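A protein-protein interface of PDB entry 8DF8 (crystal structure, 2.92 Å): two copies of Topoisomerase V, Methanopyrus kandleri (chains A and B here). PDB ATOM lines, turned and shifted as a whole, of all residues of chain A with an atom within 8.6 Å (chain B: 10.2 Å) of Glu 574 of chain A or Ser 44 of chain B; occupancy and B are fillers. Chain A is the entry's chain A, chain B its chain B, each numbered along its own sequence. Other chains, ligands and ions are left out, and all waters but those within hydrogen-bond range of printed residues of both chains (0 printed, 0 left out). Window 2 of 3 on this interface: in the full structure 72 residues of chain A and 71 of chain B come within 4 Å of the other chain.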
ATOM      1  N   ASP A 560     -21.647  15.648  35.990  1.00  0.00           N
ATOM      2  CA  ASP A 560     -21.299  14.303  35.546  1.00  0.00           C
ATOM      3  C   ASP A 560     -22.186  13.263  36.216  1.00  0.00           C
ATOM      4  O   ASP A 560     -22.550  12.255  35.599  1.00  0.00           O
ATOM      5  CB  ASP A 560     -19.825  14.019  35.830  1.00  0.00           C
ATOM      6  CG  ASP A 560     -19.408  12.624  35.409  1.00  0.00           C
ATOM      7  OD1 ASP A 560     -19.555  12.294  34.213  1.00  0.00           O
ATOM      8  OD2 ASP A 560     -18.934  11.859  36.274  1.00  0.00           O
ATOM      9  N   ALA A 563     -25.358  13.281  34.270  1.00  0.00           N
ATOM     10  CA  ALA A 563     -25.195  12.558  33.013  1.00  0.00           C
ATOM     11  C   ALA A 563     -25.158  11.051  33.238  1.00  0.00           C
ATOM     12  O   ALA A 563     -25.631  10.286  32.389  1.00  0.00           O
ATOM     13  CB  ALA A 563     -23.927  13.023  32.296  1.00  0.00           C
ATOM     14  N   ILE A 568     -26.590   9.183  29.852  1.00  0.00           N
ATOM     15  CA  ILE A 568     -26.203   9.959  28.673  1.00  0.00           C
ATOM     16  C   ILE A 568     -24.916   9.370  28.101  1.00  0.00           C
ATOM     17  O   ILE A 568     -23.942   9.193  28.849  1.00  0.00           O
ATOM     18  CB  ILE A 568     -26.019  11.429  29.032  1.00  0.00           C
ATOM     19  CG1 ILE A 568     -27.247  11.955  29.776  1.00  0.00           C
ATOM     20  CG2 ILE A 568     -25.765  12.252  27.778  1.00  0.00           C
ATOM     21  CD1 ILE A 568     -28.510  11.950  28.948  1.00  0.00           C
ATOM     22  N   PRO A 569     -24.872   9.053  26.808  1.00  0.00           N
ATOM     23  CA  PRO A 569     -23.644   8.502  26.227  1.00  0.00           C
ATOM     24  C   PRO A 569     -22.495   9.498  26.302  1.00  0.00           C
ATOM     25  O   PRO A 569     -22.688  10.704  26.472  1.00  0.00           O
ATOM     26  CB  PRO A 569     -24.036   8.212  24.773  1.00  0.00           C
ATOM     27  CG  PRO A 569     -25.530   8.103  24.796  1.00  0.00           C
ATOM     28  CD  PRO A 569     -25.983   9.074  25.843  1.00  0.00           C
ATOM     29  N   LYS A 570     -21.277   8.966  26.180  1.00  0.00           N
ATOM     30  CA  LYS A 570     -20.085   9.804  26.272  1.00  0.00           C
ATOM     31  C   LYS A 570     -20.055  10.839  25.154  1.00  0.00           C
ATOM     32  O   LYS A 570     -19.777  12.021  25.392  1.00  0.00           O
ATOM     33  CB  LYS A 570     -18.827   8.935  26.249  1.00  0.00           C
ATOM     34  CG  LYS A 570     -17.535   9.721  26.406  1.00  0.00           C
ATOM     35  CD  LYS A 570     -16.315   8.834  26.222  1.00  0.00           C
ATOM     36  CE  LYS A 570     -15.032   9.640  26.341  1.00  0.00           C
ATOM     37  NZ  LYS A 570     -13.827   8.767  26.402  1.00  0.00           N
ATOM     38  N   LYS A 571     -20.331  10.407  23.921  1.00  0.00           N
ATOM     39  CA  LYS A 571     -20.315  11.326  22.787  1.00  0.00           C
ATOM     40  C   LYS A 571     -21.335  12.443  22.974  1.00  0.00           C
ATOM     41  O   LYS A 571     -21.031  13.623  22.762  1.00  0.00           O
ATOM     42  CB  LYS A 571     -20.594  10.563  21.492  1.00  0.00           C
ATOM     43  CG  LYS A 571     -19.644   9.410  21.216  1.00  0.00           C
ATOM     44  CD  LYS A 571     -20.011   8.707  19.916  1.00  0.00           C
ATOM     45  CE  LYS A 571     -19.024   7.600  19.580  1.00  0.00           C
ATOM     46  NZ  LYS A 571     -19.323   6.970  18.263  1.00  0.00           N
ATOM     47  N   LEU A 572     -22.552  12.086  23.391  1.00  0.00           N
ATOM     48  CA  LEU A 572     -23.596  13.089  23.561  1.00  0.00           C
ATOM     49  C   LEU A 572     -23.325  13.995  24.756  1.00  0.00           C
ATOM     50  O   LEU A 572     -23.736  15.160  24.751  1.00  0.00           O
ATOM     51  CB  LEU A 572     -24.956  12.409  23.712  1.00  0.00           C
ATOM     52  CG  LEU A 572     -26.178  13.265  23.379  1.00  0.00           C
ATOM     53  CD1 LEU A 572     -26.415  13.281  21.877  1.00  0.00           C
ATOM     54  CD2 LEU A 572     -27.407  12.763  24.115  1.00  0.00           C
ATOM     55  N   ARG A 573     -22.641  13.489  25.786  1.00  0.00           N
ATOM     56  CA  ARG A 573     -22.358  14.323  26.949  1.00  0.00           C
ATOM     57  C   ARG A 573     -21.170  15.245  26.713  1.00  0.00           C
ATOM     58  O   ARG A 573     -21.082  16.306  27.342  1.00  0.00           O
ATOM     59  CB  ARG A 573     -22.115  13.454  28.187  1.00  0.00           C
ATOM     60  CG  ARG A 573     -20.655  13.356  28.613  1.00  0.00           C
ATOM     61  CD  ARG A 573     -20.508  12.666  29.959  1.00  0.00           C
ATOM     62  NE  ARG A 573     -20.889  11.261  29.888  1.00  0.00           N
ATOM     63  CZ  ARG A 573     -20.032  10.264  29.708  1.00  0.00           C
ATOM     64  NH1 ARG A 573     -18.733  10.483  29.586  1.00  0.00           N
ATOM     65  NH2 ARG A 573     -20.492   9.018  29.645  1.00  0.00           N
ATOM     66  N   GLU A 574     -20.252  14.868  25.821  1.00  0.00           N
ATOM     67  CA  GLU A 574     -19.095  15.701  25.520  1.00  0.00           C
ATOM     68  C   GLU A 574     -19.292  16.589  24.299  1.00  0.00           C
ATOM     69  O   GLU A 574     -18.483  17.496  24.078  1.00  0.00           O
ATOM     70  CB  GLU A 574     -17.848  14.829  25.317  1.00  0.00           C
ATOM     71  CG  GLU A 574     -17.346  14.150  26.582  1.00  0.00           C
ATOM     72  CD  GLU A 574     -16.097  13.324  26.343  1.00  0.00           C
ATOM     73  OE1 GLU A 574     -15.809  13.004  25.171  1.00  0.00           O
ATOM     74  OE2 GLU A 574     -15.401  12.995  27.328  1.00  0.00           O
ATOM     75  N   ALA A 575     -20.340  16.360  23.509  1.00  0.00           N
ATOM     76  CA  ALA A 575     -20.595  17.179  22.332  1.00  0.00           C
ATOM     77  C   ALA A 575     -21.514  18.364  22.607  1.00  0.00           C
ATOM     78  O   ALA A 575     -21.585  19.275  21.774  1.00  0.00           O
ATOM     79  CB  ALA A 575     -21.194  16.323  21.211  1.00  0.00           C
ATOM     80  N   PHE A 576     -22.216  18.381  23.740  1.00  0.00           N
ATOM     81  CA  PHE A 576     -23.159  19.447  24.050  1.00  0.00           C
ATOM     82  C   PHE A 576     -23.080  19.768  25.537  1.00  0.00           C
ATOM     83  O   PHE A 576     -22.243  19.230  26.269  1.00  0.00           O
ATOM     84  CB  PHE A 576     -24.591  19.054  23.667  1.00  0.00           C
ATOM     85  CG  PHE A 576     -24.731  18.555  22.258  1.00  0.00           C
ATOM     86  CD1 PHE A 576     -24.924  19.436  21.209  1.00  0.00           C
ATOM     87  CD2 PHE A 576     -24.678  17.198  21.985  1.00  0.00           C
ATOM     88  CE1 PHE A 576     -25.055  18.973  19.913  1.00  0.00           C
ATOM     89  CE2 PHE A 576     -24.809  16.730  20.692  1.00  0.00           C
ATOM     90  CZ  PHE A 576     -24.999  17.618  19.654  1.00  0.00           C
ATOM     91  N   ASP A 577     -23.961  20.660  25.979  1.00  0.00           N
ATOM     92  CA  ASP A 577     -24.147  20.936  27.394  1.00  0.00           C
ATOM     93  C   ASP A 577     -25.203  19.996  27.973  1.00  0.00           C
ATOM     94  O   ASP A 577     -25.887  19.270  27.250  1.00  0.00           O
ATOM     95  CB  ASP A 577     -24.541  22.396  27.612  1.00  0.00           C
ATOM     96  CG  ASP A 577     -25.799  22.779  26.860  1.00  0.00           C
ATOM     97  OD1 ASP A 577     -25.906  22.433  25.664  1.00  0.00           O
ATOM     98  OD2 ASP A 577     -26.682  23.424  27.464  1.00  0.00           O
ATOM     99  N   LEU A 578     -25.330  20.017  29.303  1.00  0.00           N
ATOM    100  CA  LEU A 578     -26.232  19.085  29.977  1.00  0.00           C
ATOM    101  C   LEU A 578     -27.675  19.269  29.523  1.00  0.00           C
ATOM    102  O   LEU A 578     -28.375  18.289  29.246  1.00  0.00           O
ATOM    103  CB  LEU A 578     -26.130  19.251  31.491  1.00  0.00           C
ATOM    104  CG  LEU A 578     -25.278  18.210  32.212  1.00  0.00           C
ATOM    105  CD1 LEU A 578     -23.796  18.518  32.054  1.00  0.00           C
ATOM    106  CD2 LEU A 578     -25.683  18.129  33.674  1.00  0.00           C
ATOM    107  N   ALA A 581     -28.155  18.102  25.748  1.00  0.00           N
ATOM    108  CA  ALA A 581     -27.877  16.675  25.613  1.00  0.00           C
ATOM    109  C   ALA A 581     -28.965  15.840  26.276  1.00  0.00           C
ATOM    110  O   ALA A 581     -29.469  14.874  25.687  1.00  0.00           O
ATOM    111  CB  ALA A 581     -26.508  16.344  26.204  1.00  0.00           C
ATOM    112  N   GLY A 607     -23.525  23.191  18.855  1.00  0.00           N
ATOM    113  CA  GLY A 607     -22.230  23.290  19.500  1.00  0.00           C
ATOM    114  C   GLY A 607     -21.374  22.048  19.371  1.00  0.00           C
ATOM    115  O   GLY A 607     -20.577  21.743  20.263  1.00  0.00           O
ATOM    116  N   ALA A 608     -21.519  21.325  18.265  1.00  0.00           N
ATOM    117  CA  ALA A 608     -20.812  20.068  18.056  1.00  0.00           C
ATOM    118  C   ALA A 608     -19.646  20.274  17.099  1.00  0.00           C
ATOM    119  O   ALA A 608     -19.798  20.917  16.055  1.00  0.00           O
ATOM    120  CB  ALA A 608     -21.757  18.995  17.512  1.00  0.00           C
ATOM    121  N   THR A 609     -18.487  19.735  17.466  1.00  0.00           N
ATOM    122  CA  THR A 609     -17.356  19.699  16.553  1.00  0.00           C
ATOM    123  C   THR A 609     -17.739  18.910  15.302  1.00  0.00           C
ATOM    124  O   THR A 609     -18.487  17.931  15.399  1.00  0.00           O
ATOM    125  CB  THR A 609     -16.147  19.056  17.244  1.00  0.00           C
ATOM    126  OG1 THR A 609     -15.857  19.766  18.455  1.00  0.00           O
ATOM    127  CG2 THR A 609     -14.914  19.070  16.349  1.00  0.00           C
ATOM    128  N   ALA A 612     -17.058  15.512  16.041  1.00  0.00           N
ATOM    129  CA  ALA A 612     -18.015  15.103  17.064  1.00  0.00           C
ATOM    130  C   ALA A 612     -19.421  14.995  16.489  1.00  0.00           C
ATOM    131  O   ALA A 612     -20.162  14.061  16.812  1.00  0.00           O
ATOM    132  CB  ALA A 612     -17.987  16.082  18.238  1.00  0.00           C
ATOM    133  N   GLU A 615     -19.633  11.847  14.583  1.00  0.00           N
ATOM    134  CA  GLU A 615     -19.733  10.681  15.453  1.00  0.00           C
ATOM    135  C   GLU A 615     -21.113  10.576  16.091  1.00  0.00           C
ATOM    136  O   GLU A 615     -21.577   9.467  16.375  1.00  0.00           O
ATOM    137  CB  GLU A 615     -18.649  10.726  16.529  1.00  0.00           C
ATOM    138  CG  GLU A 615     -17.240  10.521  15.993  1.00  0.00           C
ATOM    139  CD  GLU A 615     -16.273  10.054  17.063  1.00  0.00           C
ATOM    140  OE1 GLU A 615     -16.004  10.830  18.004  1.00  0.00           O
ATOM    141  OE2 GLU A 615     -15.780   8.910  16.962  1.00  0.00           O
ATOM    142  N   ILE A 616     -21.779  11.709  16.326  1.00  0.00           N
ATOM    143  CA  ILE A 616     -23.172  11.661  16.762  1.00  0.00           C
ATOM    144  C   ILE A 616     -24.044  11.085  15.653  1.00  0.00           C
ATOM    145  O   ILE A 616     -24.993  10.336  15.911  1.00  0.00           O
ATOM    146  CB  ILE A 616     -23.650  13.056  17.210  1.00  0.00           C
ATOM    147  CG1 ILE A 616     -23.491  13.225  18.724  1.00  0.00           C
ATOM    148  CG2 ILE A 616     -25.105  13.282  16.832  1.00  0.00           C
ATOM    149  CD1 ILE A 616     -22.059  13.222  19.212  1.00  0.00           C
ATOM    150  N   ARG B  37      -8.497   3.610  35.600  1.00  0.00           N
ATOM    151  CA  ARG B  37      -8.898   3.376  34.213  1.00  0.00           C
ATOM    152  C   ARG B  37     -10.200   4.104  33.883  1.00  0.00           C
ATOM    153  O   ARG B  37     -10.335   4.716  32.810  1.00  0.00           O
ATOM    154  CB  ARG B  37      -9.041   1.875  33.956  1.00  0.00           C
ATOM    155  CG  ARG B  37      -9.169   1.498  32.488  1.00  0.00           C
ATOM    156  CD  ARG B  37      -7.914   1.854  31.706  1.00  0.00           C
ATOM    157  NE  ARG B  37      -8.090   1.639  30.275  1.00  0.00           N
ATOM    158  CZ  ARG B  37      -8.599   2.537  29.442  1.00  0.00           C
ATOM    159  NH1 ARG B  37      -8.981   3.732  29.864  1.00  0.00           N
ATOM    160  NH2 ARG B  37      -8.724   2.231  28.155  1.00  0.00           N
ATOM    161  N   TYR B  38     -11.165   4.058  34.807  1.00  0.00           N
ATOM    162  CA  TYR B  38     -12.436   4.741  34.597  1.00  0.00           C
ATOM    163  C   TYR B  38     -12.233   6.242  34.453  1.00  0.00           C
ATOM    164  O   TYR B  38     -12.851   6.875  33.594  1.00  0.00           O
ATOM    165  CB  TYR B  38     -13.397   4.440  35.749  1.00  0.00           C
ATOM    166  CG  TYR B  38     -14.728   5.155  35.640  1.00  0.00           C
ATOM    167  CD1 TYR B  38     -15.778   4.600  34.922  1.00  0.00           C
ATOM    168  CD2 TYR B  38     -14.933   6.386  36.253  1.00  0.00           C
ATOM    169  CE1 TYR B  38     -16.996   5.247  34.816  1.00  0.00           C
ATOM    170  CE2 TYR B  38     -16.147   7.043  36.151  1.00  0.00           C
ATOM    171  CZ  TYR B  38     -17.174   6.468  35.431  1.00  0.00           C
ATOM    172  OH  TYR B  38     -18.385   7.115  35.329  1.00  0.00           O
ATOM    173  N   LEU B  39     -11.398   6.836  35.308  1.00  0.00           N
ATOM    174  CA  LEU B  39     -11.124   8.265  35.189  1.00  0.00           C
ATOM    175  C   LEU B  39     -10.385   8.588  33.899  1.00  0.00           C
ATOM    176  O   LEU B  39     -10.608   9.653  33.311  1.00  0.00           O
ATOM    177  CB  LEU B  39     -10.324   8.760  36.394  1.00  0.00           C
ATOM    178  CG  LEU B  39     -11.140   9.204  37.608  1.00  0.00           C
ATOM    179  CD1 LEU B  39     -10.221   9.604  38.750  1.00  0.00           C
ATOM    180  CD2 LEU B  39     -12.057  10.353  37.230  1.00  0.00           C
ATOM    181  N   MET B  40      -9.501   7.694  33.449  1.00  0.00           N
ATOM    182  CA  MET B  40      -8.790   7.925  32.195  1.00  0.00           C
ATOM    183  C   MET B  40      -9.752   7.982  31.018  1.00  0.00           C
ATOM    184  O   MET B  40      -9.598   8.819  30.122  1.00  0.00           O
ATOM    185  CB  MET B  40      -7.745   6.833  31.965  1.00  0.00           C
ATOM    186  CG  MET B  40      -6.518   6.932  32.848  1.00  0.00           C
ATOM    187  SD  MET B  40      -5.331   5.634  32.476  1.00  0.00           S
ATOM    188  CE  MET B  40      -5.000   5.983  30.752  1.00  0.00           C
ATOM    189  N   GLU B  41     -10.754   7.105  31.005  1.00  0.00           N
ATOM    190  CA  GLU B  41     -11.663   7.065  29.862  1.00  0.00           C
ATOM    191  C   GLU B  41     -12.878   7.978  29.997  1.00  0.00           C
ATOM    192  O   GLU B  41     -13.472   8.342  28.975  1.00  0.00           O
ATOM    193  CB  GLU B  41     -12.128   5.625  29.606  1.00  0.00           C
ATOM    194  CG  GLU B  41     -12.782   4.925  30.794  1.00  0.00           C
ATOM    195  CD  GLU B  41     -14.240   5.299  31.006  1.00  0.00           C
ATOM    196  OE1 GLU B  41     -14.855   5.909  30.110  1.00  0.00           O
ATOM    197  OE2 GLU B  41     -14.778   4.971  32.082  1.00  0.00           O
ATOM    198  N   ARG B  42     -13.257   8.365  31.216  1.00  0.00           N
ATOM    199  CA  ARG B  42     -14.488   9.127  31.412  1.00  0.00           C
ATOM    200  C   ARG B  42     -14.353  10.553  30.899  1.00  0.00           C
ATOM    201  O   ARG B  42     -15.289  11.094  30.298  1.00  0.00           O
ATOM    202  CB  ARG B  42     -14.865   9.129  32.894  1.00  0.00           C
ATOM    203  CG  ARG B  42     -16.205   9.773  33.215  1.00  0.00           C
ATOM    204  CD  ARG B  42     -17.371   8.946  32.697  1.00  0.00           C
ATOM    205  NE  ARG B  42     -18.651   9.589  32.969  1.00  0.00           N
ATOM    206  CZ  ARG B  42     -19.834   9.018  32.782  1.00  0.00           C
ATOM    207  NH1 ARG B  42     -19.939   7.780  32.329  1.00  0.00           N
ATOM    208  NH2 ARG B  42     -20.937   9.705  33.062  1.00  0.00           N
ATOM    209  N   SER B  43     -13.200  11.175  31.122  1.00  0.00           N
ATOM    210  CA  SER B  43     -12.940  12.543  30.697  1.00  0.00           C
ATOM    211  C   SER B  43     -11.774  12.535  29.723  1.00  0.00           C
ATOM    212  O   SER B  43     -10.725  11.948  30.008  1.00  0.00           O
ATOM    213  CB  SER B  43     -12.631  13.445  31.896  1.00  0.00           C
ATOM    214  OG  SER B  43     -12.183  14.723  31.477  1.00  0.00           O
ATOM    215  N   SER B  44     -11.963  13.183  28.571  1.00  0.00           N
ATOM    216  CA  SER B  44     -10.895  13.242  27.580  1.00  0.00           C
ATOM    217  C   SER B  44      -9.689  14.009  28.104  1.00  0.00           C
ATOM    218  O   SER B  44      -8.557  13.750  27.680  1.00  0.00           O
ATOM    219  CB  SER B  44     -11.414  13.877  26.289  1.00  0.00           C
ATOM    220  OG  SER B  44     -12.382  13.048  25.670  1.00  0.00           O
ATOM    221  N   SER B  45      -9.907  14.951  29.023  1.00  0.00           N
ATOM    222  CA  SER B  45      -8.791  15.692  29.601  1.00  0.00           C
ATOM    223  C   SER B  45      -7.969  14.817  30.540  1.00  0.00           C
ATOM    224  O   SER B  45      -6.736  14.903  30.557  1.00  0.00           O
ATOM    225  CB  SER B  45      -9.310  16.929  30.334  1.00  0.00           C
ATOM    226  OG  SER B  45      -8.242  17.701  30.855  1.00  0.00           O
ATOM    227  N   ALA B  46      -8.634  13.967  31.326  1.00  0.00           N
ATOM    228  CA  ALA B  46      -7.927  13.076  32.239  1.00  0.00           C
ATOM    229  C   ALA B  46      -7.150  11.985  31.513  1.00  0.00           C
ATOM    230  O   ALA B  46      -6.201  11.436  32.083  1.00  0.00           O
ATOM    231  CB  ALA B  46      -8.912  12.445  33.225  1.00  0.00           C
ATOM    232  N   LYS B  47      -7.533  11.653  30.278  1.00  0.00           N
ATOM    233  CA  LYS B  47      -6.801  10.642  29.519  1.00  0.00           C
ATOM    234  C   LYS B  47      -5.371  11.080  29.228  1.00  0.00           C
ATOM    235  O   LYS B  47      -4.461  10.243  29.180  1.00  0.00           O
ATOM    236  CB  LYS B  47      -7.544  10.335  28.217  1.00  0.00           C
ATOM    237  CG  LYS B  47      -6.855   9.332  27.306  1.00  0.00           C
ATOM    238  CD  LYS B  47      -7.744   8.977  26.123  1.00  0.00           C
ATOM    239  CE  LYS B  47      -7.111   7.909  25.247  1.00  0.00           C
ATOM    240  NZ  LYS B  47      -8.011   7.510  24.128  1.00  0.00           N
ATOM    241  N   ASN B  48      -5.152  12.382  29.039  1.00  0.00           N
ATOM    242  CA  ASN B  48      -3.832  12.915  28.732  1.00  0.00           C
ATOM    243  C   ASN B  48      -2.981  13.178  29.968  1.00  0.00           C
ATOM    244  O   ASN B  48      -1.750  13.217  29.856  1.00  0.00           O
ATOM    245  CB  ASN B  48      -3.966  14.214  27.930  1.00  0.00           C
ATOM    246  CG  ASN B  48      -4.835  14.047  26.696  1.00  0.00           C
ATOM    247  OD1 ASN B  48      -4.729  13.054  25.975  1.00  0.00           O
ATOM    248  ND2 ASN B  48      -5.705  15.021  26.449  1.00  0.00           N
ATOM    249  N   ASP B  49      -3.603  13.368  31.131  1.00  0.00           N
ATOM    250  CA  ASP B  49      -2.875  13.742  32.339  1.00  0.00           C
ATOM    251  C   ASP B  49      -1.870  12.664  32.729  1.00  0.00           C
ATOM    252  O   ASP B  49      -2.236  11.502  32.931  1.00  0.00           O
ATOM    253  CB  ASP B  49      -3.862  13.992  33.479  1.00  0.00           C
ATOM    254  CG  ASP B  49      -3.262  14.816  34.606  1.00  0.00           C
ATOM    255  OD1 ASP B  49      -2.022  14.821  34.758  1.00  0.00           O
ATOM    256  OD2 ASP B  49      -4.036  15.464  35.342  1.00  0.00           O
ATOM    257  N   GLU B  50      -0.597  13.057  32.830  1.00  0.00           N
ATOM    258  CA  GLU B  50       0.443  12.130  33.268  1.00  0.00           C
ATOM    259  C   GLU B  50       0.287  11.749  34.734  1.00  0.00           C
ATOM    260  O   GLU B  50       0.661  10.637  35.124  1.00  0.00           O
ATOM    261  CB  GLU B  50       1.826  12.740  33.030  1.00  0.00           C
ATOM    262  CG  GLU B  50       2.340  12.578  31.613  1.00  0.00           C
ATOM    263  CD  GLU B  50       2.576  11.125  31.250  1.00  0.00           C
ATOM    264  OE1 GLU B  50       3.587  10.555  31.712  1.00  0.00           O
ATOM    265  OE2 GLU B  50       1.752  10.554  30.506  1.00  0.00           O
ATOM    266  N   LEU B  52      -2.381  11.040  36.374  1.00  0.00           N
ATOM    267  CA  LEU B  52      -3.287   9.902  36.484  1.00  0.00           C
ATOM    268  C   LEU B  52      -2.612   8.604  36.049  1.00  0.00           C
ATOM    269  O   LEU B  52      -2.883   7.538  36.616  1.00  0.00           O
ATOM    270  CB  LEU B  52      -4.550  10.167  35.665  1.00  0.00           C
ATOM    271  CG  LEU B  52      -5.706   9.171  35.759  1.00  0.00           C
ATOM    272  CD1 LEU B  52      -6.063   8.886  37.207  1.00  0.00           C
ATOM    273  CD2 LEU B  52      -6.912   9.721  35.019  1.00  0.00           C
ATOM    274  N   TYR B 268     -11.774  16.310  37.951  1.00  0.00           N
ATOM    275  CA  TYR B 268     -12.296  16.029  36.619  1.00  0.00           C
ATOM    276  C   TYR B 268     -13.790  15.737  36.588  1.00  0.00           C
ATOM    277  O   TYR B 268     -14.399  15.836  35.517  1.00  0.00           O
ATOM    278  CB  TYR B 268     -11.545  14.852  35.984  1.00  0.00           C
ATOM    279  CG  TYR B 268     -10.150  15.202  35.519  1.00  0.00           C
ATOM    280  CD1 TYR B 268      -9.944  15.836  34.301  1.00  0.00           C
ATOM    281  CD2 TYR B 268      -9.040  14.901  36.297  1.00  0.00           C
ATOM    282  CE1 TYR B 268      -8.671  16.161  33.871  1.00  0.00           C
ATOM    283  CE2 TYR B 268      -7.763  15.220  35.875  1.00  0.00           C
ATOM    284  CZ  TYR B 268      -7.585  15.850  34.661  1.00  0.00           C
ATOM    285  OH  TYR B 268      -6.315  16.170  34.236  1.00  0.00           O
ATOM    286  N   LEU B 269     -14.395  15.377  37.721  1.00  0.00           N
ATOM    287  CA  LEU B 269     -15.813  15.054  37.762  1.00  0.00           C
ATOM    288  C   LEU B 269     -16.606  15.872  38.770  1.00  0.00           C
ATOM    289  O   LEU B 269     -17.842  15.820  38.737  1.00  0.00           O
ATOM    290  CB  LEU B 269     -16.017  13.561  38.073  1.00  0.00           C
ATOM    291  CG  LEU B 269     -15.259  12.545  37.217  1.00  0.00           C
ATOM    292  CD1 LEU B 269     -15.588  11.132  37.672  1.00  0.00           C
ATOM    293  CD2 LEU B 269     -15.577  12.727  35.742  1.00  0.00           C
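The side-chain carboxylate (OD1) of Asp 560 of chain A is in salt-bridge range of the guanidinium group (NE) of Arg 42 of chain B, 3.1 Å away.
The backbone carbonyl oxygen (O) of Glu 41 of chain B lies within hydrogen-bond range of the side-chain amino group (NZ) of Lys 570 of chain A (2.6 Å).
The side-chain carboxylate of Glu 574 of chain A is in hydrogen-bond range of the side-chain hydroxyl of Ser 44 of chain B, 3.4 Å away.
NH2 of Arg 573 of chain A sits close to NH1 of Arg 42 of chain B, 3.0 Å away.
NE of Arg 42 of chain B sits close to OH of Tyr 38 of chain B.
O of Ser 44 of chain B lies within hydrogen-bond range of ND2 of Asn 48 of chain B, 3.4 Å away.
Among the printed residues, pairs that only touch across the chains: Asp 560 of chain A with Leu 269 of chain B (3.5 Å) and Glu 574 of chain A with Arg 42 of chain B (3.5 Å).
Lys 570 of chain A touches just one residue of chain B: Glu 41.
Of chain B, only Arg 42 and Ser 44 come within 4 Å of Glu 574 of chain A.
No residue of chain B comes within 4 Å of Ala 575 of chain A.
Printed residues of chain A within 4 Å of Arg 42 of chain B: Asp 560 (3.1 Å), Arg 573 (3.0 Å) and Glu 574 (3.5 Å).
No residue of chain A comes within 4 Å of Ser 43 of chain B.
Ser 44 of chain B touches one residue of chain A.
Asp 49 of chain B touches none of the printed residues of chain A.
Of the printed residues of chain A, Leu 269 of chain B touches Asp 560 (3.5 Å).
The nearest residue of chain B that does not touch Glu 574 of chain A is Ser 43 of chain B (4.2 Å).
Printed residues of chain A that touch a printed residue of chain B: Asp 560, Lys 570, Arg 573 and Glu 574.
Of the 17 printed residues of chain B, 4 touch a printed residue of chain A.
Hydrophobic or aromatic side chains of chain B within 4 Å of the printed part of chain A: Leu 269.
No position is printed for both chains.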
